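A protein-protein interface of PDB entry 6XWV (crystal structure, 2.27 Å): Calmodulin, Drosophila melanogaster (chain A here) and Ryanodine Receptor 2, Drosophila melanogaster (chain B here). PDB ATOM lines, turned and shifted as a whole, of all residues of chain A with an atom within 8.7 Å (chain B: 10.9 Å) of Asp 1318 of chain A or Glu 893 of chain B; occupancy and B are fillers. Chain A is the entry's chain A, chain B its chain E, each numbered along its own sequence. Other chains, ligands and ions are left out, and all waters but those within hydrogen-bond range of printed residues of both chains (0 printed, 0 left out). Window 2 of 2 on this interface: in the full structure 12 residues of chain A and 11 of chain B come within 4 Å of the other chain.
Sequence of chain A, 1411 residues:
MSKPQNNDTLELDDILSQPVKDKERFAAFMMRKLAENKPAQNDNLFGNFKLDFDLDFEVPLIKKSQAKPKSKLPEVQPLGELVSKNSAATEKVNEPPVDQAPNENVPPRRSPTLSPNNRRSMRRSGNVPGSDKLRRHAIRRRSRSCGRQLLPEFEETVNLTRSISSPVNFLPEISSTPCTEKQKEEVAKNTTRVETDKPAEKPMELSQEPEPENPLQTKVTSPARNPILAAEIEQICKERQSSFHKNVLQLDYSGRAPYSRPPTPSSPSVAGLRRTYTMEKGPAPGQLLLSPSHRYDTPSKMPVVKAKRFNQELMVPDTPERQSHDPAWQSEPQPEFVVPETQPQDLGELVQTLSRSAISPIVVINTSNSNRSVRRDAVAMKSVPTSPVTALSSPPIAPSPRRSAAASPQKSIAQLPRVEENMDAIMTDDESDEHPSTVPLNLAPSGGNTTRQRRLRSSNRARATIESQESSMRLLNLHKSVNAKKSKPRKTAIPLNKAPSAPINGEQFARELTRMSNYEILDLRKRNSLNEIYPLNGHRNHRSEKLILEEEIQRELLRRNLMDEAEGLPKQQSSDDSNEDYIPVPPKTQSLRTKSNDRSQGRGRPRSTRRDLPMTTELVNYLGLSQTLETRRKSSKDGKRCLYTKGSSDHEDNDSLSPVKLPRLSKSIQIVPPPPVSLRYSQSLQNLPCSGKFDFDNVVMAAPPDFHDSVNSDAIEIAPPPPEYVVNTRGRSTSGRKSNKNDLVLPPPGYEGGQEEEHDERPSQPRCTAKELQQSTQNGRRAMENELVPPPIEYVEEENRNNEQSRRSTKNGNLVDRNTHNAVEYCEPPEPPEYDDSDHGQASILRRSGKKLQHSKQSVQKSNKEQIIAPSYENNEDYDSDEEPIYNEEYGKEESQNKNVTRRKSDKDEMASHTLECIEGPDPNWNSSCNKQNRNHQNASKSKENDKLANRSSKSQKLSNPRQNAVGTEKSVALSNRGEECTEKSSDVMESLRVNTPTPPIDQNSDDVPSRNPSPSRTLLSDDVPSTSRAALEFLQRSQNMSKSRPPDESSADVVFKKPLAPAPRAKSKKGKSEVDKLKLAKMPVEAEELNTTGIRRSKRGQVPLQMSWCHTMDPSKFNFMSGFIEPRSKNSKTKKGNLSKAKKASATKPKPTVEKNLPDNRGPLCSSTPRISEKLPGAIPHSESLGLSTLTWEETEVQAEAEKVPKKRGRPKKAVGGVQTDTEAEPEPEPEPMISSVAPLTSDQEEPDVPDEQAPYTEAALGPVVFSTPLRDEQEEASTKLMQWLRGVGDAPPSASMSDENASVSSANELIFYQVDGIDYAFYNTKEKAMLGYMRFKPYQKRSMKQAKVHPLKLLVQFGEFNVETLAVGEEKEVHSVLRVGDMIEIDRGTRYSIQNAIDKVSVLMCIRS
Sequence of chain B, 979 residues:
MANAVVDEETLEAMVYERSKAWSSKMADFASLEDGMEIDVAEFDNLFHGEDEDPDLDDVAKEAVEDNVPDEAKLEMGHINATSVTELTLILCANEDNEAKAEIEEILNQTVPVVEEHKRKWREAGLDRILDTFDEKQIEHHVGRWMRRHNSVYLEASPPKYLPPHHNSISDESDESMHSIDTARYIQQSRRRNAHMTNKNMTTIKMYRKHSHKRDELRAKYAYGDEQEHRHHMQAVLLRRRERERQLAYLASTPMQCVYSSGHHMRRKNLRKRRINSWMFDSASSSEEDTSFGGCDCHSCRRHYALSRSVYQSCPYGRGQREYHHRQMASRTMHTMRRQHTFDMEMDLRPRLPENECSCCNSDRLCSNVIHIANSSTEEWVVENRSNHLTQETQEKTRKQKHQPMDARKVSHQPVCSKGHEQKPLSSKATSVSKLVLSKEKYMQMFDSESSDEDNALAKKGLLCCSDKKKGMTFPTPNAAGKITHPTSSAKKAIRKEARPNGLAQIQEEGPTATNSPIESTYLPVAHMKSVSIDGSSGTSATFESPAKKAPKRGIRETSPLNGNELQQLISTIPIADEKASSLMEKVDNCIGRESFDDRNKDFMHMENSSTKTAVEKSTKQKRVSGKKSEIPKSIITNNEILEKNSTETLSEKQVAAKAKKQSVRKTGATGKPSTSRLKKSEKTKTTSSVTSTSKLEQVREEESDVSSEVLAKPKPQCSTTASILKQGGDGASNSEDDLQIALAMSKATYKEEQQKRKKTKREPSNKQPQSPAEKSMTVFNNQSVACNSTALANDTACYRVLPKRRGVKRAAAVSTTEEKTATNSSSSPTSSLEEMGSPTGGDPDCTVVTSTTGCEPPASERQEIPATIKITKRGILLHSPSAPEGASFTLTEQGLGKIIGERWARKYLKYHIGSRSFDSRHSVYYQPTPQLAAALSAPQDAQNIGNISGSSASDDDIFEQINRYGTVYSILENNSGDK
The backbone carbonyl oxygen (O) of Gln 1316 of chain A is in hydrogen-bond range of the backbone NH (N) of Thr 890 of chain B, at 3.4 Å. O of Gln 1316 of chain A sits at hydrogen-bond distance from N of Leu 891 of chain B (3.0 Å).
O of Tyr 1322 of chain A is in hydrogen-bond range of N of Tyr 1315 of chain A (2.7 Å).
Among the printed residues, pairs that only touch across the chains: Tyr 1315 of chain A with Leu 891 of chain B, Tyr 1315 of chain A with Leu 896 of chain B, Tyr 1315 of chain A with Ile 899 of chain B, Val 1317 of chain A with Leu 891 of chain B, Val 1317 of chain A with Glu 893 of chain B and Asp 1318 of chain A with Glu 893 of chain B.
Printed residues of chain B within 4 Å of Tyr 1315 of chain A: Leu 891 (3.5 Å), Leu 896 (3.8 Å) and Ile 899 (3.6 Å). Of the printed residues of chain B, Gln 1316 of chain A touches Thr 890 and Leu 891. Val 1317 of chain A touches two residues of chain B. Printed residues of chain B within 4 Å of Asp 1318 of chain A: Glu 893. No residue of chain B comes within 4 Å of Gly 1319 of chain A. No residue of chain A comes within 4 Å of Thr 892 of chain B. Of chain A, only Val 1317 and Asp 1318 come within 4 Å of Glu 893 of chain B. No residue of chain A comes within 4 Å of Gln 894 of chain B. Printed residues of chain A within 4 Å of Ile 899 of chain B: Tyr 1315 (3.6 Å). The nearest residue of chain B that does not touch Asp 1318 of chain A is Leu 891 of chain B (4.3 Å). The nearest printed residue of chain A that does not touch Thr 890 of chain B is Tyr 1315 of chain A (4.4 Å).
Of the 12 printed residues of chain B, 5 touch a printed residue of chain A. Hydrophobic or aromatic side chains of chain B within 4 Å of the printed part of chain A: Leu 891, Leu 896 and Ile 899. Among the printed residues, 8 pairs touch across the chains. Among the printed residues, no Asp or Glu carboxylate lies within 4 Å of a Lys or Arg side-chain nitrogen of the other chain.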
ATOM      1  N   TYR A1315      28.771 -13.745   2.687  1.00  0.00           N
ATOM      2  CA  TYR A1315      27.610 -14.618   2.563  1.00  0.00           C
ATOM      3  C   TYR A1315      28.072 -15.997   2.109  1.00  0.00           C
ATOM      4  O   TYR A1315      28.857 -16.110   1.160  1.00  0.00           O
ATOM      5  CB  TYR A1315      26.591 -14.050   1.567  1.00  0.00           C
ATOM      6  CG  TYR A1315      26.180 -12.618   1.854  1.00  0.00           C
ATOM      7  CD1 TYR A1315      25.028 -12.334   2.578  1.00  0.00           C
ATOM      8  CD2 TYR A1315      26.950 -11.549   1.407  1.00  0.00           C
ATOM      9  CE1 TYR A1315      24.650 -11.025   2.840  1.00  0.00           C
ATOM     10  CE2 TYR A1315      26.583 -10.243   1.666  1.00  0.00           C
ATOM     11  CZ  TYR A1315      25.435  -9.984   2.384  1.00  0.00           C
ATOM     12  OH  TYR A1315      25.070  -8.682   2.640  1.00  0.00           O
ATOM     13  N   GLN A1316      27.596 -17.042   2.776  1.00  0.00           N
ATOM     14  CA  GLN A1316      27.933 -18.400   2.370  1.00  0.00           C
ATOM     15  C   GLN A1316      26.926 -18.835   1.312  1.00  0.00           C
ATOM     16  O   GLN A1316      25.720 -18.894   1.581  1.00  0.00           O
ATOM     17  CB  GLN A1316      27.931 -19.359   3.561  1.00  0.00           C
ATOM     18  CG  GLN A1316      28.558 -20.709   3.234  1.00  0.00           C
ATOM     19  CD  GLN A1316      28.356 -21.746   4.324  1.00  0.00           C
ATOM     20  OE1 GLN A1316      27.539 -22.657   4.185  1.00  0.00           O
ATOM     21  NE2 GLN A1316      29.109 -21.620   5.409  1.00  0.00           N
ATOM     22  N   VAL A1317      27.423 -19.141   0.116  1.00  0.00           N
ATOM     23  CA  VAL A1317      26.595 -19.570  -1.003  1.00  0.00           C
ATOM     24  C   VAL A1317      27.204 -20.839  -1.584  1.00  0.00           C
ATOM     25  O   VAL A1317      28.374 -20.841  -1.989  1.00  0.00           O
ATOM     26  CB  VAL A1317      26.478 -18.480  -2.082  1.00  0.00           C
ATOM     27  CG1 VAL A1317      25.612 -18.960  -3.231  1.00  0.00           C
ATOM     28  CG2 VAL A1317      25.917 -17.193  -1.491  1.00  0.00           C
ATOM     29  N   ASP A1318      26.416 -21.915  -1.616  1.00  0.00           N
ATOM     30  CA  ASP A1318      26.871 -23.208  -2.132  1.00  0.00           C
ATOM     31  C   ASP A1318      28.138 -23.676  -1.415  1.00  0.00           C
ATOM     32  O   ASP A1318      29.032 -24.278  -2.013  1.00  0.00           O
ATOM     33  CB  ASP A1318      27.081 -23.148  -3.648  1.00  0.00           C
ATOM     34  CG  ASP A1318      25.787 -22.882  -4.405  1.00  0.00           C
ATOM     35  OD1 ASP A1318      24.712 -23.300  -3.920  1.00  0.00           O
ATOM     36  OD2 ASP A1318      25.844 -22.244  -5.480  1.00  0.00           O
ATOM     37  N   GLY A1319      28.214 -23.384  -0.116  1.00  0.00           N
ATOM     38  CA  GLY A1319      29.310 -23.801   0.730  1.00  0.00           C
ATOM     39  C   GLY A1319      30.560 -22.947   0.677  1.00  0.00           C
ATOM     40  O   GLY A1319      31.534 -23.271   1.370  1.00  0.00           O
ATOM     41  N   ILE A1320      30.580 -21.885  -0.123  1.00  0.00           N
ATOM     42  CA  ILE A1320      31.738 -21.005  -0.247  1.00  0.00           C
ATOM     43  C   ILE A1320      31.360 -19.606   0.229  1.00  0.00           C
ATOM     44  O   ILE A1320      30.242 -19.140  -0.020  1.00  0.00           O
ATOM     45  CB  ILE A1320      32.279 -20.986  -1.691  1.00  0.00           C
ATOM     46  CG1 ILE A1320      32.877 -22.359  -2.027  1.00  0.00           C
ATOM     47  CG2 ILE A1320      33.320 -19.887  -1.881  1.00  0.00           C
ATOM     48  CD1 ILE A1320      33.931 -22.330  -3.108  1.00  0.00           C
ATOM     49  N   ASP A1321      32.289 -18.946   0.922  1.00  0.00           N
ATOM     50  CA  ASP A1321      32.065 -17.608   1.455  1.00  0.00           C
ATOM     51  C   ASP A1321      32.380 -16.550   0.401  1.00  0.00           C
ATOM     52  O   ASP A1321      33.472 -16.543  -0.178  1.00  0.00           O
ATOM     53  CB  ASP A1321      32.927 -17.378   2.697  1.00  0.00           C
ATOM     54  CG  ASP A1321      32.368 -18.055   3.933  1.00  0.00           C
ATOM     55  OD1 ASP A1321      31.169 -18.401   3.929  1.00  0.00           O
ATOM     56  OD2 ASP A1321      33.124 -18.236   4.915  1.00  0.00           O
ATOM     57  N   TYR A1322      31.426 -15.650   0.168  1.00  0.00           N
ATOM     58  CA  TYR A1322      31.565 -14.582  -0.814  1.00  0.00           C
ATOM     59  C   TYR A1322      31.352 -13.229  -0.148  1.00  0.00           C
ATOM     60  O   TYR A1322      30.422 -13.056   0.649  1.00  0.00           O
ATOM     61  CB  TYR A1322      30.561 -14.727  -1.965  1.00  0.00           C
ATOM     62  CG  TYR A1322      30.752 -15.948  -2.831  1.00  0.00           C
ATOM     63  CD1 TYR A1322      31.408 -15.860  -4.053  1.00  0.00           C
ATOM     64  CD2 TYR A1322      30.265 -17.187  -2.436  1.00  0.00           C
ATOM     65  CE1 TYR A1322      31.584 -16.976  -4.850  1.00  0.00           C
ATOM     66  CE2 TYR A1322      30.432 -18.307  -3.228  1.00  0.00           C
ATOM     67  CZ  TYR A1322      31.091 -18.196  -4.434  1.00  0.00           C
ATOM     68  OH  TYR A1322      31.262 -19.310  -5.224  1.00  0.00           O
ATOM     69  N   PHE A1324      31.337  -9.136  -1.583  1.00  0.00           N
ATOM     70  CA  PHE A1324      31.421  -8.224  -2.713  1.00  0.00           C
ATOM     71  C   PHE A1324      31.333  -6.793  -2.204  1.00  0.00           C
ATOM     72  O   PHE A1324      30.660  -6.517  -1.206  1.00  0.00           O
ATOM     73  CB  PHE A1324      30.296  -8.472  -3.728  1.00  0.00           C
ATOM     74  CG  PHE A1324      30.501  -9.695  -4.578  1.00  0.00           C
ATOM     75  CD1 PHE A1324      31.501  -9.732  -5.537  1.00  0.00           C
ATOM     76  CD2 PHE A1324      29.691 -10.805  -4.416  1.00  0.00           C
ATOM     77  CE1 PHE A1324      31.688 -10.857  -6.320  1.00  0.00           C
ATOM     78  CE2 PHE A1324      29.871 -11.936  -5.195  1.00  0.00           C
ATOM     79  CZ  PHE A1324      30.871 -11.963  -6.150  1.00  0.00           C
ATOM     80  N   LYS A1339      37.779 -22.662   2.503  1.00  0.00           N
ATOM     81  CA  LYS A1339      38.137 -23.490   3.627  1.00  0.00           C
ATOM     82  C   LYS A1339      39.295 -24.403   3.248  1.00  0.00           C
ATOM     83  O   LYS A1339      39.592 -24.579   2.068  1.00  0.00           O
ATOM     84  CB  LYS A1339      37.019 -24.472   3.941  1.00  0.00           C
ATOM     85  CG  LYS A1339      35.514 -24.272   4.048  1.00  0.00           C
ATOM     86  CD  LYS A1339      35.272 -24.679   5.509  1.00  0.00           C
ATOM     87  CE  LYS A1339      33.977 -25.468   5.897  1.00  0.00           C
ATOM     88  NZ  LYS A1339      32.784 -24.634   5.589  1.00  0.00           N
ATOM     89  N   GLN A1342      39.288 -26.924   0.175  1.00  0.00           N
ATOM     90  CA  GLN A1342      38.009 -26.822  -0.505  1.00  0.00           C
ATOM     91  C   GLN A1342      38.220 -26.522  -1.980  1.00  0.00           C
ATOM     92  O   GLN A1342      39.103 -25.745  -2.354  1.00  0.00           O
ATOM     93  CB  GLN A1342      37.157 -25.727   0.138  1.00  0.00           C
ATOM     94  CG  GLN A1342      35.721 -25.681  -0.368  1.00  0.00           C
ATOM     95  CD  GLN A1342      34.822 -24.814   0.491  1.00  0.00           C
ATOM     96  OE1 GLN A1342      35.279 -23.855   1.107  1.00  0.00           O
ATOM     97  NE2 GLN A1342      33.536 -25.150   0.537  1.00  0.00           N
ATOM     98  N   LYS A1343      37.402 -27.147  -2.817  1.00  0.00           N
ATOM     99  CA  LYS A1343      37.456 -26.972  -4.257  1.00  0.00           C
ATOM    100  C   LYS A1343      36.096 -26.499  -4.745  1.00  0.00           C
ATOM    101  O   LYS A1343      35.059 -26.916  -4.213  1.00  0.00           O
ATOM    102  CB  LYS A1343      37.852 -28.279  -4.967  1.00  0.00           C
ATOM    103  CG  LYS A1343      37.880 -28.170  -6.486  1.00  0.00           C
ATOM    104  CD  LYS A1343      38.115 -29.523  -7.149  1.00  0.00           C
ATOM    105  CE  LYS A1343      37.524 -29.555  -8.550  1.00  0.00           C
ATOM    106  NZ  LYS A1343      38.509 -30.009  -9.571  1.00  0.00           N
ATOM    107  N   ARG A1344      36.095 -25.649  -5.766  1.00  0.00           N
ATOM    108  CA  ARG A1344      34.864 -25.261  -6.440  1.00  0.00           C
ATOM    109  C   ARG A1344      34.886 -25.856  -7.840  1.00  0.00           C
ATOM    110  O   ARG A1344      35.791 -25.562  -8.630  1.00  0.00           O
ATOM    111  CB  ARG A1344      34.706 -23.742  -6.495  1.00  0.00           C
ATOM    112  CG  ARG A1344      33.339 -23.306  -7.002  1.00  0.00           C
ATOM    113  CD  ARG A1344      33.162 -21.802  -7.009  1.00  0.00           C
ATOM    114  NE  ARG A1344      33.534 -21.232  -8.297  1.00  0.00           N
ATOM    115  CZ  ARG A1344      32.939 -20.180  -8.847  1.00  0.00           C
ATOM    116  NH1 ARG A1344      31.933 -19.583  -8.220  1.00  0.00           N
ATOM    117  NH2 ARG A1344      33.343 -19.728 -10.024  1.00  0.00           N
ATOM    118  N   SER A1345      33.890 -26.688  -8.137  1.00  0.00           N
ATOM    119  CA  SER A1345      33.814 -27.398  -9.405  1.00  0.00           C
ATOM    120  C   SER A1345      33.831 -26.427 -10.582  1.00  0.00           C
ATOM    121  O   SER A1345      33.457 -25.258 -10.469  1.00  0.00           O
ATOM    122  CB  SER A1345      32.564 -28.270  -9.453  1.00  0.00           C
ATOM    123  OG  SER A1345      32.323 -28.851  -8.184  1.00  0.00           O
ATOM    124  N   LYS A1347      33.268 -24.133 -13.624  1.00  0.00           N
ATOM    125  CA  LYS A1347      32.179 -23.286 -14.090  1.00  0.00           C
ATOM    126  C   LYS A1347      32.665 -22.518 -15.310  1.00  0.00           C
ATOM    127  O   LYS A1347      33.861 -22.478 -15.606  1.00  0.00           O
ATOM    128  CB  LYS A1347      31.702 -22.303 -13.009  1.00  0.00           C
ATOM    129  CG  LYS A1347      31.754 -22.835 -11.594  1.00  0.00           C
ATOM    130  CD  LYS A1347      30.604 -23.786 -11.323  1.00  0.00           C
ATOM    131  CE  LYS A1347      29.399 -23.048 -10.768  1.00  0.00           C
ATOM    132  NZ  LYS A1347      28.535 -23.930  -9.938  1.00  0.00           N
ATOM    133  N   ARG A1410      35.791  -8.904 -12.114  1.00  0.00           N
ATOM    134  CA  ARG A1410      35.018  -9.090 -13.337  1.00  0.00           C
ATOM    135  C   ARG A1410      35.108  -7.866 -14.240  1.00  0.00           C
ATOM    136  O   ARG A1410      35.195  -6.736 -13.762  1.00  0.00           O
ATOM    137  CB  ARG A1410      33.557  -9.389 -13.000  1.00  0.00           C
ATOM    138  CG  ARG A1410      33.288 -10.857 -12.733  1.00  0.00           C
ATOM    139  CD  ARG A1410      31.891 -11.090 -12.187  1.00  0.00           C
ATOM    140  NE  ARG A1410      30.850 -10.649 -13.110  1.00  0.00           N
ATOM    141  CZ  ARG A1410      29.551 -10.684 -12.833  1.00  0.00           C
ATOM    142  NH1 ARG A1410      29.136 -11.144 -11.661  1.00  0.00           N
ATOM    143  NH2 ARG A1410      28.666 -10.265 -13.728  1.00  0.00           N
ATOM    144  N   THR B 890      24.477 -20.270   4.470  1.00  0.00           N
ATOM    145  CA  THR B 890      23.573 -19.302   5.082  1.00  0.00           C
ATOM    146  C   THR B 890      22.661 -18.623   4.051  1.00  0.00           C
ATOM    147  O   THR B 890      21.707 -17.940   4.422  1.00  0.00           O
ATOM    148  CB  THR B 890      24.361 -18.224   5.867  1.00  0.00           C
ATOM    149  OG1 THR B 890      24.921 -17.266   4.956  1.00  0.00           O
ATOM    150  CG2 THR B 890      25.475 -18.861   6.697  1.00  0.00           C
ATOM    151  N   LEU B 891      22.943 -18.828   2.765  1.00  0.00           N
ATOM    152  CA  LEU B 891      22.155 -18.208   1.704  1.00  0.00           C
ATOM    153  C   LEU B 891      22.171 -19.089   0.462  1.00  0.00           C
ATOM    154  O   LEU B 891      23.067 -19.915   0.273  1.00  0.00           O
ATOM    155  CB  LEU B 891      22.671 -16.806   1.351  1.00  0.00           C
ATOM    156  CG  LEU B 891      22.241 -15.601   2.191  1.00  0.00           C
ATOM    157  CD1 LEU B 891      23.281 -15.252   3.253  1.00  0.00           C
ATOM    158  CD2 LEU B 891      21.941 -14.406   1.282  1.00  0.00           C
ATOM    159  N   THR B 892      21.165 -18.884  -0.386  1.00  0.00           N
ATOM    160  CA  THR B 892      21.073 -19.460  -1.720  1.00  0.00           C
ATOM    161  C   THR B 892      21.533 -18.438  -2.756  1.00  0.00           C
ATOM    162  O   THR B 892      21.675 -17.249  -2.461  1.00  0.00           O
ATOM    163  CB  THR B 892      19.637 -19.904  -2.021  1.00  0.00           C
ATOM    164  OG1 THR B 892      19.489 -20.147  -3.426  1.00  0.00           O
ATOM    165  CG2 THR B 892      18.639 -18.836  -1.588  1.00  0.00           C
ATOM    166  N   GLU B 893      21.769 -18.910  -3.986  1.00  0.00           N
ATOM    167  CA  GLU B 893      22.253 -17.989  -5.015  1.00  0.00           C
ATOM    168  C   GLU B 893      21.181 -16.978  -5.406  1.00  0.00           C
ATOM    169  O   GLU B 893      21.483 -15.797  -5.620  1.00  0.00           O
ATOM    170  CB  GLU B 893      22.750 -18.741  -6.250  1.00  0.00           C
ATOM    171  CG  GLU B 893      23.286 -17.791  -7.328  1.00  0.00           C
ATOM    172  CD  GLU B 893      24.377 -18.398  -8.191  1.00  0.00           C
ATOM    173  OE1 GLU B 893      24.653 -19.608  -8.052  1.00  0.00           O
ATOM    174  OE2 GLU B 893      24.981 -17.650  -8.991  1.00  0.00           O
ATOM    175  N   GLN B 894      19.921 -17.413  -5.504  1.00  0.00           N
ATOM    176  CA  GLN B 894      18.838 -16.456  -5.701  1.00  0.00           C
ATOM    177  C   GLN B 894      18.718 -15.523  -4.502  1.00  0.00           C
ATOM    178  O   GLN B 894      18.397 -14.338  -4.655  1.00  0.00           O
ATOM    179  CB  GLN B 894      17.522 -17.191  -5.949  1.00  0.00           C
ATOM    180  N   GLY B 895      18.991 -16.039  -3.301  1.00  0.00           N
ATOM    181  CA  GLY B 895      18.917 -15.207  -2.113  1.00  0.00           C
ATOM    182  C   GLY B 895      20.012 -14.158  -2.059  1.00  0.00           C
ATOM    183  O   GLY B 895      19.775 -13.022  -1.638  1.00  0.00           O
ATOM    184  N   LEU B 896      21.230 -14.523  -2.469  1.00  0.00           N
ATOM    185  CA  LEU B 896      22.296 -13.529  -2.558  1.00  0.00           C
ATOM    186  C   LEU B 896      21.959 -12.462  -3.589  1.00  0.00           C
ATOM    187  O   LEU B 896      22.268 -11.281  -3.394  1.00  0.00           O
ATOM    188  CB  LEU B 896      23.628 -14.196  -2.900  1.00  0.00           C
ATOM    189  CG  LEU B 896      24.771 -13.206  -3.171  1.00  0.00           C
ATOM    190  CD1 LEU B 896      25.486 -12.840  -1.881  1.00  0.00           C
ATOM    191  CD2 LEU B 896      25.752 -13.747  -4.201  1.00  0.00           C
ATOM    192  N   GLY B 897      21.322 -12.860  -4.692  1.00  0.00           N
ATOM    193  CA  GLY B 897      20.918 -11.886  -5.692  1.00  0.00           C
ATOM    194  C   GLY B 897      19.972 -10.838  -5.138  1.00  0.00           C
ATOM    195  O   GLY B 897      20.074  -9.655  -5.477  1.00  0.00           O
ATOM    196  N   LYS B 898      19.043 -11.255  -4.274  1.00  0.00           N
ATOM    197  CA  LYS B 898      18.112 -10.298  -3.683  1.00  0.00           C
ATOM    198  C   LYS B 898      18.799  -9.436  -2.631  1.00  0.00           C
ATOM    199  O   LYS B 898      18.563  -8.223  -2.565  1.00  0.00           O
ATOM    200  CB  LYS B 898      16.916 -11.029  -3.074  1.00  0.00           C
ATOM    201  N   ILE B 899      19.645 -10.044  -1.795  1.00  0.00           N
ATOM    202  CA  ILE B 899      20.333  -9.288  -0.752  1.00  0.00           C
ATOM    203  C   ILE B 899      21.265  -8.253  -1.371  1.00  0.00           C
ATOM    204  O   ILE B 899      21.312  -7.098  -0.929  1.00  0.00           O
ATOM    205  CB  ILE B 899      21.083 -10.241   0.199  1.00  0.00           C
ATOM    206  CG1 ILE B 899      20.099 -11.194   0.882  1.00  0.00           C
ATOM    207  CG2 ILE B 899      21.864  -9.451   1.244  1.00  0.00           C
ATOM    208  CD1 ILE B 899      18.866 -10.512   1.440  1.00  0.00           C
ATOM    209  N   ILE B 900      22.013  -8.644  -2.406  1.00  0.00           N
ATOM    210  CA  ILE B 900      22.823  -7.672  -3.136  1.00  0.00           C
ATOM    211  C   ILE B 900      21.929  -6.635  -3.804  1.00  0.00           C
ATOM    212  O   ILE B 900      22.282  -5.452  -3.887  1.00  0.00           O
ATOM    213  CB  ILE B 900      23.725  -8.383  -4.159  1.00  0.00           C
ATOM    214  CG1 ILE B 900      24.721  -9.304  -3.450  1.00  0.00           C
ATOM    215  CG2 ILE B 900      24.469  -7.369  -5.024  1.00  0.00           C
ATOM    216  CD1 ILE B 900      25.688  -8.577  -2.539  1.00  0.00           C
ATOM    217  N   GLY B 901      20.755  -7.058  -4.281  1.00  0.00           N
ATOM    218  CA  GLY B 901      19.851  -6.122  -4.929  1.00  0.00           C
ATOM    219  C   GLY B 901      19.303  -5.077  -3.977  1.00  0.00           C
ATOM    220  O   GLY B 901      19.197  -3.897  -4.331  1.00  0.00           O
